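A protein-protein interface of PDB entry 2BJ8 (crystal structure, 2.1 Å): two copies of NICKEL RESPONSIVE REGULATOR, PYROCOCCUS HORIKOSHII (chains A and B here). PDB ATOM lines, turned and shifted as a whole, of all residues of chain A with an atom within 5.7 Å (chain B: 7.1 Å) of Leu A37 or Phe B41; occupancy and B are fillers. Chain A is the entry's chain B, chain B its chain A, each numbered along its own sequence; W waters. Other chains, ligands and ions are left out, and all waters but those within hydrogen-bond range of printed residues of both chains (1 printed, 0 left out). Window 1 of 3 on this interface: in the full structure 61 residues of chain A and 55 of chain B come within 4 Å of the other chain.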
ATOM      1  N   PHE A  18     -28.273  14.697   6.170  1.00  0.00           N
ATOM      2  CA  PHE A  18     -28.659  15.774   5.264  1.00  0.00           C
ATOM      3  C   PHE A  18     -29.137  17.017   6.027  1.00  0.00           C
ATOM      4  O   PHE A  18     -28.688  18.130   5.747  1.00  0.00           O
ATOM      5  CB  PHE A  18     -29.765  15.288   4.321  1.00  0.00           C
ATOM      6  CG  PHE A  18     -30.160  16.297   3.270  1.00  0.00           C
ATOM      7  CD1 PHE A  18     -29.214  16.801   2.378  1.00  0.00           C
ATOM      8  CD2 PHE A  18     -31.477  16.734   3.164  1.00  0.00           C
ATOM      9  CE1 PHE A  18     -29.577  17.724   1.399  1.00  0.00           C
ATOM     10  CE2 PHE A  18     -31.848  17.659   2.186  1.00  0.00           C
ATOM     11  CZ  PHE A  18     -30.896  18.154   1.302  1.00  0.00           C
ATOM     12  N   ILE A  21     -26.289  18.930   7.630  1.00  0.00           N
ATOM     13  CA  ILE A  21     -25.483  19.678   6.676  1.00  0.00           C
ATOM     14  C   ILE A  21     -26.146  20.950   6.147  1.00  0.00           C
ATOM     15  O   ILE A  21     -25.563  22.034   6.223  1.00  0.00           O
ATOM     16  CB  ILE A  21     -25.075  18.790   5.475  1.00  0.00           C
ATOM     17  CG1 ILE A  21     -24.086  17.724   5.942  1.00  0.00           C
ATOM     18  CG2 ILE A  21     -24.451  19.637   4.374  1.00  0.00           C
ATOM     19  CD1 ILE A  21     -23.536  16.867   4.829  1.00  0.00           C
ATOM     20  N   ILE A  22     -27.358  20.831   5.614  1.00  0.00           N
ATOM     21  CA  ILE A  22     -28.025  22.008   5.068  1.00  0.00           C
ATOM     22  C   ILE A  22     -28.215  23.122   6.094  1.00  0.00           C
ATOM     23  O   ILE A  22     -28.231  24.305   5.734  1.00  0.00           O
ATOM     24  CB  ILE A  22     -29.389  21.664   4.449  1.00  0.00           C
ATOM     25  CG1 ILE A  22     -30.358  21.190   5.530  1.00  0.00           C
ATOM     26  CG2 ILE A  22     -29.205  20.615   3.364  1.00  0.00           C
ATOM     27  CD1 ILE A  22     -31.742  20.920   5.003  1.00  0.00           C
ATOM     28  N   ILE A  25     -24.848  24.839   6.317  1.00  0.00           N
ATOM     29  CA  ILE A  25     -24.641  25.617   5.098  1.00  0.00           C
ATOM     30  C   ILE A  25     -25.447  26.915   5.132  1.00  0.00           C
ATOM     31  O   ILE A  25     -24.968  27.963   4.696  1.00  0.00           O
ATOM     32  CB  ILE A  25     -25.057  24.825   3.843  1.00  0.00           C
ATOM     33  CG1 ILE A  25     -24.043  23.714   3.566  1.00  0.00           C
ATOM     34  CG2 ILE A  25     -25.160  25.763   2.645  1.00  0.00           C
ATOM     35  CD1 ILE A  25     -24.396  22.852   2.357  1.00  0.00           C
ATOM     36  N   TYR A  27     -29.271  26.767   4.637  1.00  0.00           N
ATOM     37  CA  TYR A  27     -30.607  26.620   4.069  1.00  0.00           C
ATOM     38  C   TYR A  27     -31.639  26.822   5.172  1.00  0.00           C
ATOM     39  O   TYR A  27     -31.410  26.460   6.329  1.00  0.00           O
ATOM     40  CB  TYR A  27     -30.808  25.236   3.448  1.00  0.00           C
ATOM     41  CG  TYR A  27     -30.137  25.041   2.108  1.00  0.00           C
ATOM     42  CD1 TYR A  27     -28.819  24.591   2.022  1.00  0.00           C
ATOM     43  CD2 TYR A  27     -30.820  25.313   0.923  1.00  0.00           C
ATOM     44  CE1 TYR A  27     -28.197  24.413   0.786  1.00  0.00           C
ATOM     45  CE2 TYR A  27     -30.209  25.141  -0.318  1.00  0.00           C
ATOM     46  CZ  TYR A  27     -28.898  24.693  -0.379  1.00  0.00           C
ATOM     47  OH  TYR A  27     -28.285  24.543  -1.602  1.00  0.00           O
ATOM     48  N   GLU A  32     -36.604  23.362   0.654  1.00  0.00           N
ATOM     49  CA  GLU A  32     -35.898  24.273  -0.229  1.00  0.00           C
ATOM     50  C   GLU A  32     -34.627  23.609  -0.773  1.00  0.00           C
ATOM     51  O   GLU A  32     -34.316  23.726  -1.956  1.00  0.00           O
ATOM     52  CB  GLU A  32     -35.536  25.557   0.523  1.00  0.00           C
ATOM     53  CG  GLU A  32     -35.105  26.678  -0.394  1.00  0.00           C
ATOM     54  CD  GLU A  32     -36.200  27.067  -1.373  1.00  0.00           C
ATOM     55  OE1 GLU A  32     -35.906  27.175  -2.582  1.00  0.00           O
ATOM     56  OE2 GLU A  32     -37.354  27.268  -0.930  1.00  0.00           O
ATOM     57  N   ALA A  33     -33.902  22.914   0.097  1.00  0.00           N
ATOM     58  CA  ALA A  33     -32.669  22.239  -0.300  1.00  0.00           C
ATOM     59  C   ALA A  33     -32.943  21.132  -1.311  1.00  0.00           C
ATOM     60  O   ALA A  33     -32.190  20.955  -2.271  1.00  0.00           O
ATOM     61  CB  ALA A  33     -31.972  21.664   0.923  1.00  0.00           C
ATOM     62  N   ILE A  34     -34.026  20.391  -1.105  1.00  0.00           N
ATOM     63  CA  ILE A  34     -34.360  19.307  -2.014  1.00  0.00           C
ATOM     64  C   ILE A  34     -34.797  19.847  -3.369  1.00  0.00           C
ATOM     65  O   ILE A  34     -34.436  19.283  -4.404  1.00  0.00           O
ATOM     66  CB  ILE A  34     -35.452  18.396  -1.417  1.00  0.00           C
ATOM     67  CG1 ILE A  34     -34.881  17.637  -0.219  1.00  0.00           C
ATOM     68  CG2 ILE A  34     -35.937  17.396  -2.459  1.00  0.00           C
ATOM     69  CD1 ILE A  34     -35.895  16.756   0.491  1.00  0.00           C
ATOM     70  N   ARG A  35     -35.575  20.927  -3.373  1.00  0.00           N
ATOM     71  CA  ARG A  35     -35.994  21.518  -4.638  1.00  0.00           C
ATOM     72  C   ARG A  35     -34.734  22.000  -5.364  1.00  0.00           C
ATOM     73  O   ARG A  35     -34.643  21.909  -6.590  1.00  0.00           O
ATOM     74  CB  ARG A  35     -36.976  22.680  -4.417  1.00  0.00           C
ATOM     75  CG  ARG A  35     -38.395  22.233  -4.045  1.00  0.00           C
ATOM     76  CD  ARG A  35     -39.409  23.375  -4.167  1.00  0.00           C
ATOM     77  NE  ARG A  35     -39.196  24.407  -3.154  1.00  0.00           N
ATOM     78  CZ  ARG A  35     -39.587  24.305  -1.887  1.00  0.00           C
ATOM     79  NH1 ARG A  35     -39.340  25.290  -1.037  1.00  0.00           N
ATOM     80  NH2 ARG A  35     -40.243  23.228  -1.472  1.00  0.00           N
ATOM     81  N   ASP A  36     -33.760  22.502  -4.607  1.00  0.00           N
ATOM     82  CA  ASP A  36     -32.501  22.952  -5.202  1.00  0.00           C
ATOM     83  C   ASP A  36     -31.782  21.761  -5.846  1.00  0.00           C
ATOM     84  O   ASP A  36     -31.200  21.885  -6.919  1.00  0.00           O
ATOM     85  CB  ASP A  36     -31.577  23.570  -4.147  1.00  0.00           C
ATOM     86  CG  ASP A  36     -31.859  25.042  -3.900  1.00  0.00           C
ATOM     87  OD1 ASP A  36     -31.122  25.655  -3.095  1.00  0.00           O
ATOM     88  OD2 ASP A  36     -32.808  25.585  -4.504  1.00  0.00           O
ATOM     89  N   LEU A  37     -31.819  20.610  -5.182  1.00  0.00           N
ATOM     90  CA  LEU A  37     -31.171  19.419  -5.714  1.00  0.00           C
ATOM     91  C   LEU A  37     -31.840  19.001  -7.010  1.00  0.00           C
ATOM     92  O   LEU A  37     -31.171  18.593  -7.959  1.00  0.00           O
ATOM     93  CB  LEU A  37     -31.253  18.255  -4.724  1.00  0.00           C
ATOM     94  CG  LEU A  37     -30.459  18.396  -3.424  1.00  0.00           C
ATOM     95  CD1 LEU A  37     -30.608  17.127  -2.594  1.00  0.00           C
ATOM     96  CD2 LEU A  37     -29.011  18.646  -3.745  1.00  0.00           C
ATOM     97  N   ILE A  38     -33.165  19.101  -7.045  1.00  0.00           N
ATOM     98  CA  ILE A  38     -33.911  18.712  -8.226  1.00  0.00           C
ATOM     99  C   ILE A  38     -33.620  19.655  -9.388  1.00  0.00           C
ATOM    100  O   ILE A  38     -33.521  19.217 -10.534  1.00  0.00           O
ATOM    101  CB  ILE A  38     -35.428  18.643  -7.916  1.00  0.00           C
ATOM    102  CG1 ILE A  38     -35.689  17.443  -6.996  1.00  0.00           C
ATOM    103  CG2 ILE A  38     -36.234  18.527  -9.202  1.00  0.00           C
ATOM    104  CD1 ILE A  38     -37.109  17.345  -6.454  1.00  0.00           C
ATOM    105  N   ARG A  39     -33.467  20.943  -9.097  1.00  0.00           N
ATOM    106  CA  ARG A  39     -33.149  21.902 -10.147  1.00  0.00           C
ATOM    107  C   ARG A  39     -31.750  21.599 -10.683  1.00  0.00           C
ATOM    108  O   ARG A  39     -31.511  21.653 -11.893  1.00  0.00           O
ATOM    109  CB  ARG A  39     -33.190  23.342  -9.616  1.00  0.00           C
ATOM    110  CG  ARG A  39     -34.562  24.002  -9.653  1.00  0.00           C
ATOM    111  CD  ARG A  39     -34.455  25.497  -9.335  1.00  0.00           C
ATOM    112  NE  ARG A  39     -34.290  25.741  -7.908  1.00  0.00           N
ATOM    113  CZ  ARG A  39     -35.299  25.863  -7.052  1.00  0.00           C
ATOM    114  NH1 ARG A  39     -36.548  25.774  -7.484  1.00  0.00           N
ATOM    115  NH2 ARG A  39     -35.059  26.044  -5.761  1.00  0.00           N
ATOM    116  N   ASP A  40     -30.827  21.273  -9.783  1.00  0.00           N
ATOM    117  CA  ASP A  40     -29.464  20.966 -10.199  1.00  0.00           C
ATOM    118  C   ASP A  40     -29.459  19.748 -11.123  1.00  0.00           C
ATOM    119  O   ASP A  40     -28.811  19.750 -12.168  1.00  0.00           O
ATOM    120  CB  ASP A  40     -28.571  20.702  -8.983  1.00  0.00           C
ATOM    121  CG  ASP A  40     -27.159  20.272  -9.381  1.00  0.00           C
ATOM    122  OD1 ASP A  40     -26.473  21.054 -10.066  1.00  0.00           O
ATOM    123  OD2 ASP A  40     -26.733  19.152  -9.017  1.00  0.00           O
ATOM    124  N   PHE A  41     -30.197  18.717 -10.728  1.00  0.00           N
ATOM    125  CA  PHE A  41     -30.301  17.477 -11.495  1.00  0.00           C
ATOM    126  C   PHE A  41     -30.864  17.738 -12.894  1.00  0.00           C
ATOM    127  O   PHE A  41     -30.413  17.158 -13.882  1.00  0.00           O
ATOM    128  CB  PHE A  41     -31.190  16.499 -10.717  1.00  0.00           C
ATOM    129  CG  PHE A  41     -31.408  15.178 -11.396  1.00  0.00           C
ATOM    130  CD1 PHE A  41     -32.607  14.909 -12.046  1.00  0.00           C
ATOM    131  CD2 PHE A  41     -30.438  14.179 -11.335  1.00  0.00           C
ATOM    132  CE1 PHE A  41     -32.844  13.653 -12.623  1.00  0.00           C
ATOM    133  CE2 PHE A  41     -30.660  12.926 -11.908  1.00  0.00           C
ATOM    134  CZ  PHE A  41     -31.866  12.661 -12.553  1.00  0.00           C
ATOM    135  N   ILE A  42     -31.850  18.621 -12.979  1.00  0.00           N
ATOM    136  CA  ILE A  42     -32.461  18.956 -14.258  1.00  0.00           C
ATOM    137  C   ILE A  42     -31.481  19.752 -15.125  1.00  0.00           C
ATOM    138  O   ILE A  42     -31.429  19.580 -16.343  1.00  0.00           O
ATOM    139  CB  ILE A  42     -33.748  19.783 -14.045  1.00  0.00           C
ATOM    140  CG1 ILE A  42     -34.810  18.918 -13.366  1.00  0.00           C
ATOM    141  CG2 ILE A  42     -34.274  20.303 -15.368  1.00  0.00           C
ATOM    142  CD1 ILE A  42     -36.073  19.670 -13.047  1.00  0.00           C
ATOM    143  N   PHE B  18     -38.689  16.548 -13.909  1.00  0.00           N
ATOM    144  CA  PHE B  18     -38.001  15.597 -13.047  1.00  0.00           C
ATOM    145  C   PHE B  18     -38.524  14.185 -13.281  1.00  0.00           C
ATOM    146  O   PHE B  18     -37.740  13.234 -13.396  1.00  0.00           O
ATOM    147  CB  PHE B  18     -38.203  15.983 -11.578  1.00  0.00           C
ATOM    148  CG  PHE B  18     -37.473  15.099 -10.601  1.00  0.00           C
ATOM    149  CD1 PHE B  18     -36.079  15.079 -10.558  1.00  0.00           C
ATOM    150  CD2 PHE B  18     -38.181  14.321  -9.688  1.00  0.00           C
ATOM    151  CE1 PHE B  18     -35.398  14.294  -9.610  1.00  0.00           C
ATOM    152  CE2 PHE B  18     -37.509  13.535  -8.735  1.00  0.00           C
ATOM    153  CZ  PHE B  18     -36.118  13.524  -8.695  1.00  0.00           C
ATOM    154  N   ILE B  34     -34.338  10.905  -5.398  1.00  0.00           N
ATOM    155  CA  ILE B  34     -34.023  11.951  -4.444  1.00  0.00           C
ATOM    156  C   ILE B  34     -33.029  11.440  -3.412  1.00  0.00           C
ATOM    157  O   ILE B  34     -32.152  12.184  -2.963  1.00  0.00           O
ATOM    158  CB  ILE B  34     -35.322  12.511  -3.803  1.00  0.00           C
ATOM    159  CG1 ILE B  34     -36.116  13.256  -4.880  1.00  0.00           C
ATOM    160  CG2 ILE B  34     -34.991  13.462  -2.666  1.00  0.00           C
ATOM    161  CD1 ILE B  34     -37.544  13.587  -4.507  1.00  0.00           C
ATOM    162  N   ARG B  35     -33.152  10.172  -3.041  1.00  0.00           N
ATOM    163  CA  ARG B  35     -32.199   9.565  -2.105  1.00  0.00           C
ATOM    164  C   ARG B  35     -30.790   9.719  -2.711  1.00  0.00           C
ATOM    165  O   ARG B  35     -29.838  10.120  -2.032  1.00  0.00           O
ATOM    166  CB  ARG B  35     -32.493   8.068  -1.938  1.00  0.00           C
ATOM    167  CG  ARG B  35     -31.429   7.285  -1.158  1.00  0.00           C
ATOM    168  CD  ARG B  35     -31.509   5.807  -1.505  1.00  0.00           C
ATOM    169  NE  ARG B  35     -31.234   5.595  -2.929  1.00  0.00           N
ATOM    170  CZ  ARG B  35     -31.735   4.600  -3.659  1.00  0.00           C
ATOM    171  NH1 ARG B  35     -32.547   3.705  -3.112  1.00  0.00           N
ATOM    172  NH2 ARG B  35     -31.440   4.509  -4.947  1.00  0.00           N
ATOM    173  N   ASP B  36     -30.657   9.399  -3.994  1.00  0.00           N
ATOM    174  CA  ASP B  36     -29.347   9.508  -4.640  1.00  0.00           C
ATOM    175  C   ASP B  36     -28.847  10.949  -4.714  1.00  0.00           C
ATOM    176  O   ASP B  36     -27.652  11.205  -4.528  1.00  0.00           O
ATOM    177  CB  ASP B  36     -29.370   8.887  -6.041  1.00  0.00           C
ATOM    178  CG  ASP B  36     -29.563   7.373  -6.007  1.00  0.00           C
ATOM    179  OD1 ASP B  36     -29.290   6.756  -4.954  1.00  0.00           O
ATOM    180  OD2 ASP B  36     -29.977   6.794  -7.036  1.00  0.00           O
ATOM    181  N   LEU B  37     -29.753  11.895  -4.969  1.00  0.00           N
ATOM    182  CA  LEU B  37     -29.362  13.304  -5.043  1.00  0.00           C
ATOM    183  C   LEU B  37     -28.880  13.774  -3.679  1.00  0.00           C
ATOM    184  O   LEU B  37     -27.943  14.563  -3.578  1.00  0.00           O
ATOM    185  CB  LEU B  37     -30.536  14.177  -5.482  1.00  0.00           C
ATOM    186  CG  LEU B  37     -31.158  13.869  -6.843  1.00  0.00           C
ATOM    187  CD1 LEU B  37     -32.273  14.871  -7.120  1.00  0.00           C
ATOM    188  CD2 LEU B  37     -30.093  13.939  -7.928  1.00  0.00           C
ATOM    189  N   ILE B  38     -29.525  13.288  -2.625  1.00  0.00           N
ATOM    190  CA  ILE B  38     -29.146  13.670  -1.266  1.00  0.00           C
ATOM    191  C   ILE B  38     -27.786  13.090  -0.896  1.00  0.00           C
ATOM    192  O   ILE B  38     -26.950  13.780  -0.304  1.00  0.00           O
ATOM    193  CB  ILE B  38     -30.220  13.203  -0.241  1.00  0.00           C
ATOM    194  CG1 ILE B  38     -31.475  14.072  -0.388  1.00  0.00           C
ATOM    195  CG2 ILE B  38     -29.676  13.269   1.179  1.00  0.00           C
ATOM    196  CD1 ILE B  38     -32.635  13.649   0.488  1.00  0.00           C
ATOM    197  N   ARG B  39     -27.553  11.825  -1.242  1.00  0.00           N
ATOM    198  CA  ARG B  39     -26.272  11.197  -0.925  1.00  0.00           C
ATOM    199  C   ARG B  39     -25.117  11.925  -1.604  1.00  0.00           C
ATOM    200  O   ARG B  39     -24.099  12.219  -0.972  1.00  0.00           O
ATOM    201  CB  ARG B  39     -26.258   9.728  -1.345  1.00  0.00           C
ATOM    202  CG  ARG B  39     -24.996   8.988  -0.879  1.00  0.00           C
ATOM    203  CD  ARG B  39     -24.982   7.522  -1.314  1.00  0.00           C
ATOM    204  NE  ARG B  39     -25.045   7.391  -2.768  1.00  0.00           N
ATOM    205  CZ  ARG B  39     -26.123   7.009  -3.449  1.00  0.00           C
ATOM    206  NH1 ARG B  39     -27.248   6.705  -2.808  1.00  0.00           N
ATOM    207  NH2 ARG B  39     -26.079   6.956  -4.778  1.00  0.00           N
ATOM    208  N   ASP B  40     -25.274  12.227  -2.889  1.00  0.00           N
ATOM    209  CA  ASP B  40     -24.219  12.921  -3.628  1.00  0.00           C
ATOM    210  C   ASP B  40     -23.942  14.274  -3.012  1.00  0.00           C
ATOM    211  O   ASP B  40     -22.792  14.701  -2.913  1.00  0.00           O
ATOM    212  CB  ASP B  40     -24.622  13.101  -5.089  1.00  0.00           C
ATOM    213  CG  ASP B  40     -24.699  11.787  -5.830  1.00  0.00           C
ATOM    214  OD1 ASP B  40     -25.314  11.757  -6.915  1.00  0.00           O
ATOM    215  OD2 ASP B  40     -24.136  10.786  -5.331  1.00  0.00           O
ATOM    216  N   PHE B  41     -25.007  14.945  -2.593  1.00  0.00           N
ATOM    217  CA  PHE B  41     -24.885  16.257  -1.980  1.00  0.00           C
ATOM    218  C   PHE B  41     -24.070  16.182  -0.691  1.00  0.00           C
ATOM    219  O   PHE B  41     -23.202  17.018  -0.443  1.00  0.00           O
ATOM    220  CB  PHE B  41     -26.274  16.815  -1.672  1.00  0.00           C
ATOM    221  CG  PHE B  41     -26.253  18.175  -1.056  1.00  0.00           C
ATOM    222  CD1 PHE B  41     -26.161  19.313  -1.853  1.00  0.00           C
ATOM    223  CD2 PHE B  41     -26.345  18.325   0.325  1.00  0.00           C
ATOM    224  CE1 PHE B  41     -26.165  20.584  -1.281  1.00  0.00           C
ATOM    225  CE2 PHE B  41     -26.348  19.592   0.909  1.00  0.00           C
ATOM    226  CZ  PHE B  41     -26.262  20.724   0.105  1.00  0.00           C
ATOM    227  N   ILE B  42     -24.362  15.185   0.139  1.00  0.00           N
ATOM    228  CA  ILE B  42     -23.639  15.024   1.395  1.00  0.00           C
ATOM    229  C   ILE B  42     -22.157  14.781   1.117  1.00  0.00           C
ATOM    230  O   ILE B  42     -21.284  15.359   1.765  1.00  0.00           O
ATOM    231  CB  ILE B  42     -24.201  13.841   2.208  1.00  0.00           C
ATOM    232  CG1 ILE B  42     -25.601  14.192   2.725  1.00  0.00           C
ATOM    233  CG2 ILE B  42     -23.250  13.487   3.356  1.00  0.00           C
ATOM    234  CD1 ILE B  42     -26.312  13.038   3.398  1.00  0.00           C
ATOM    235  N   ILE B  43     -21.873  13.925   0.144  1.00  0.00           N
ATOM    236  CA  ILE B  43     -20.492  13.617  -0.202  1.00  0.00           C
ATOM    237  C   ILE B  43     -19.726  14.862  -0.665  1.00  0.00           C
ATOM    238  O   ILE B  43     -18.607  15.115  -0.217  1.00  0.00           O
ATOM    239  CB  ILE B  43     -20.439  12.515  -1.293  1.00  0.00           C
ATOM    240  CG1 ILE B  43     -20.940  11.193  -0.699  1.00  0.00           C
ATOM    241  CG2 ILE B  43     -19.021  12.372  -1.839  1.00  0.00           C
ATOM    242  CD1 ILE B  43     -21.116  10.074  -1.707  1.00  0.00           C
ATOM    243  N   ARG B  44     -20.336  15.648  -1.547  1.00  0.00           N
ATOM    244  CA  ARG B  44     -19.688  16.853  -2.053  1.00  0.00           C
ATOM    245  C   ARG B  44     -19.483  17.892  -0.964  1.00  0.00           C
ATOM    246  O   ARG B  44     -18.550  18.689  -1.022  1.00  0.00           O
ATOM    247  CB  ARG B  44     -20.521  17.491  -3.161  1.00  0.00           C
ATOM    248  CG  ARG B  44     -20.890  16.574  -4.292  1.00  0.00           C
ATOM    249  CD  ARG B  44     -21.454  17.393  -5.432  1.00  0.00           C
ATOM    250  NE  ARG B  44     -22.732  18.029  -5.151  1.00  0.00           N
ATOM    251  CZ  ARG B  44     -23.904  17.431  -5.313  1.00  0.00           C
ATOM    252  NH1 ARG B  44     -23.954  16.180  -5.754  1.00  0.00           N
ATOM    253  NH2 ARG B  44     -25.023  18.085  -5.045  1.00  0.00           N
ATOM    254  N   HIS B  45     -20.362  17.887   0.027  1.00  0.00           N
ATOM    255  CA  HIS B  45     -20.272  18.857   1.099  1.00  0.00           C
ATOM    256  C   HIS B  45     -19.560  18.330   2.327  1.00  0.00           C
ATOM    257  O   HIS B  45     -19.672  18.896   3.413  1.00  0.00           O
ATOM    258  CB  HIS B  45     -21.673  19.360   1.446  1.00  0.00           C
ATOM    259  CG  HIS B  45     -22.254  20.260   0.401  1.00  0.00           C
ATOM    260  ND1 HIS B  45     -22.059  21.624   0.402  1.00  0.00           N
ATOM    261  CD2 HIS B  45     -22.977  19.985  -0.710  1.00  0.00           C
ATOM    262  CE1 HIS B  45     -22.637  22.151  -0.662  1.00  0.00           C
ATOM    263  NE2 HIS B  45     -23.201  21.178  -1.355  1.00  0.00           N
ATOM    264  N   GLU B  46     -18.822  17.240   2.147  1.00  0.00           N
ATOM    265  CA  GLU B  46     -18.056  16.652   3.237  1.00  0.00           C
ATOM    266  C   GLU B  46     -16.563  16.733   2.940  1.00  0.00           C
ATOM    267  O   GLU B  46     -15.744  16.694   3.860  1.00  0.00           O
ATOM    268  CB  GLU B  46     -18.477  15.200   3.480  1.00  0.00           C
ATOM    269  CG  GLU B  46     -19.636  15.078   4.463  1.00  0.00           C
ATOM    270  CD  GLU B  46     -20.030  13.641   4.749  1.00  0.00           C
ATOM    271  OE1 GLU B  46     -20.828  13.427   5.689  1.00  0.00           O
ATOM    272  OE2 GLU B  46     -19.549  12.730   4.035  1.00  0.00           O
ATOM    273  N   ASP B 115     -21.501  29.210   0.695  1.00  0.00           N
ATOM    274  CA  ASP B 115     -22.662  28.501   1.224  1.00  0.00           C
ATOM    275  C   ASP B 115     -23.823  29.447   1.495  1.00  0.00           C
ATOM    276  O   ASP B 115     -24.973  29.129   1.197  1.00  0.00           O
ATOM    277  CB  ASP B 115     -22.302  27.750   2.511  1.00  0.00           C
ATOM    278  CG  ASP B 115     -21.435  26.532   2.250  1.00  0.00           C
ATOM    279  OD1 ASP B 115     -21.726  25.790   1.286  1.00  0.00           O
ATOM    280  OD2 ASP B 115     -20.473  26.308   3.014  1.00  0.00           O
HETATM  281  O   HOH W   1     -24.224  18.740  -8.233  1.00  0.00           O
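Phe A18 touches Ile B38, and with the chains exchanged Ile A38 touches Phe B18. Phe A18 touches Phe B41, and with the chains exchanged Phe A41 touches Phe B18. Leu B37 touches its own counterpart, Leu A37. Leu A37 touches Phe B41, and with the chains exchanged Phe A41 touches Leu B37.
Leu A37 touches just these residues of chain B: Leu B37 (3.8 Å), Ile B38 (3.9 Å) and Phe B41 (3.5 Å). Of chain A, only Phe A18, Ile A21, Ile A22, Ile A25 and Leu A37 come within 4 Å of Phe B41. Of the printed residues of chain A, His B45 touches Ile A25. Of the printed residues of chain A, Leu B37 touches Leu A37 (3.8 Å) and Phe A41 (3.4 Å). Printed residues of chain B within 4 Å of Ile A22: Phe B41. Printed residues of chain B within 4 Å of Ile A25: Phe B41, His B45 and Asp B115. The nearest residue of chain A that does not touch Phe B41 is Tyr A27 (4.2 Å).
O of Ile A22 sits at hydrogen-bond distance from N of Tyr A27 (2.9 Å).
Phe A18 touches Ile B42. Ile A21 touches Phe B41 (CG2 to CE2, 3.95 Å). Ile B42 touches Ile A21. Ile A22 touches Phe B41. Ile A25 touches Phe B41. Leu A37 touches Leu B37. Phe B41 touches Leu A37 (CD1 to CD2, 3.5 Å). Phe B18 touches Ile A38 (CD1 to CG2, 3.7 Å). Phe A41 touches Phe B18 (CD1 to CE1, 3.8 Å). Phe A41 touches Leu B37.
Water W1 bridges the side-chain carboxylate of Asp A40 (2.7 Å) and the guanidinium group of Arg B44 (3.4 Å).
Printed residues of chain B that touch a printed residue of chain A: Phe B18, Leu B37, Ile B38, Phe B41, Ile B42, His B45 and Asp B115. Hydrophobic or aromatic side chains of chain B that line the printed part of chain A: Phe B18, Leu B37, Ile B38, Phe B41, Ile B42 and His B45. Of the 16 printed residues of chain A, 7 touch a printed residue of chain B. Among the printed residues, 15 pairs touch across the chains.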
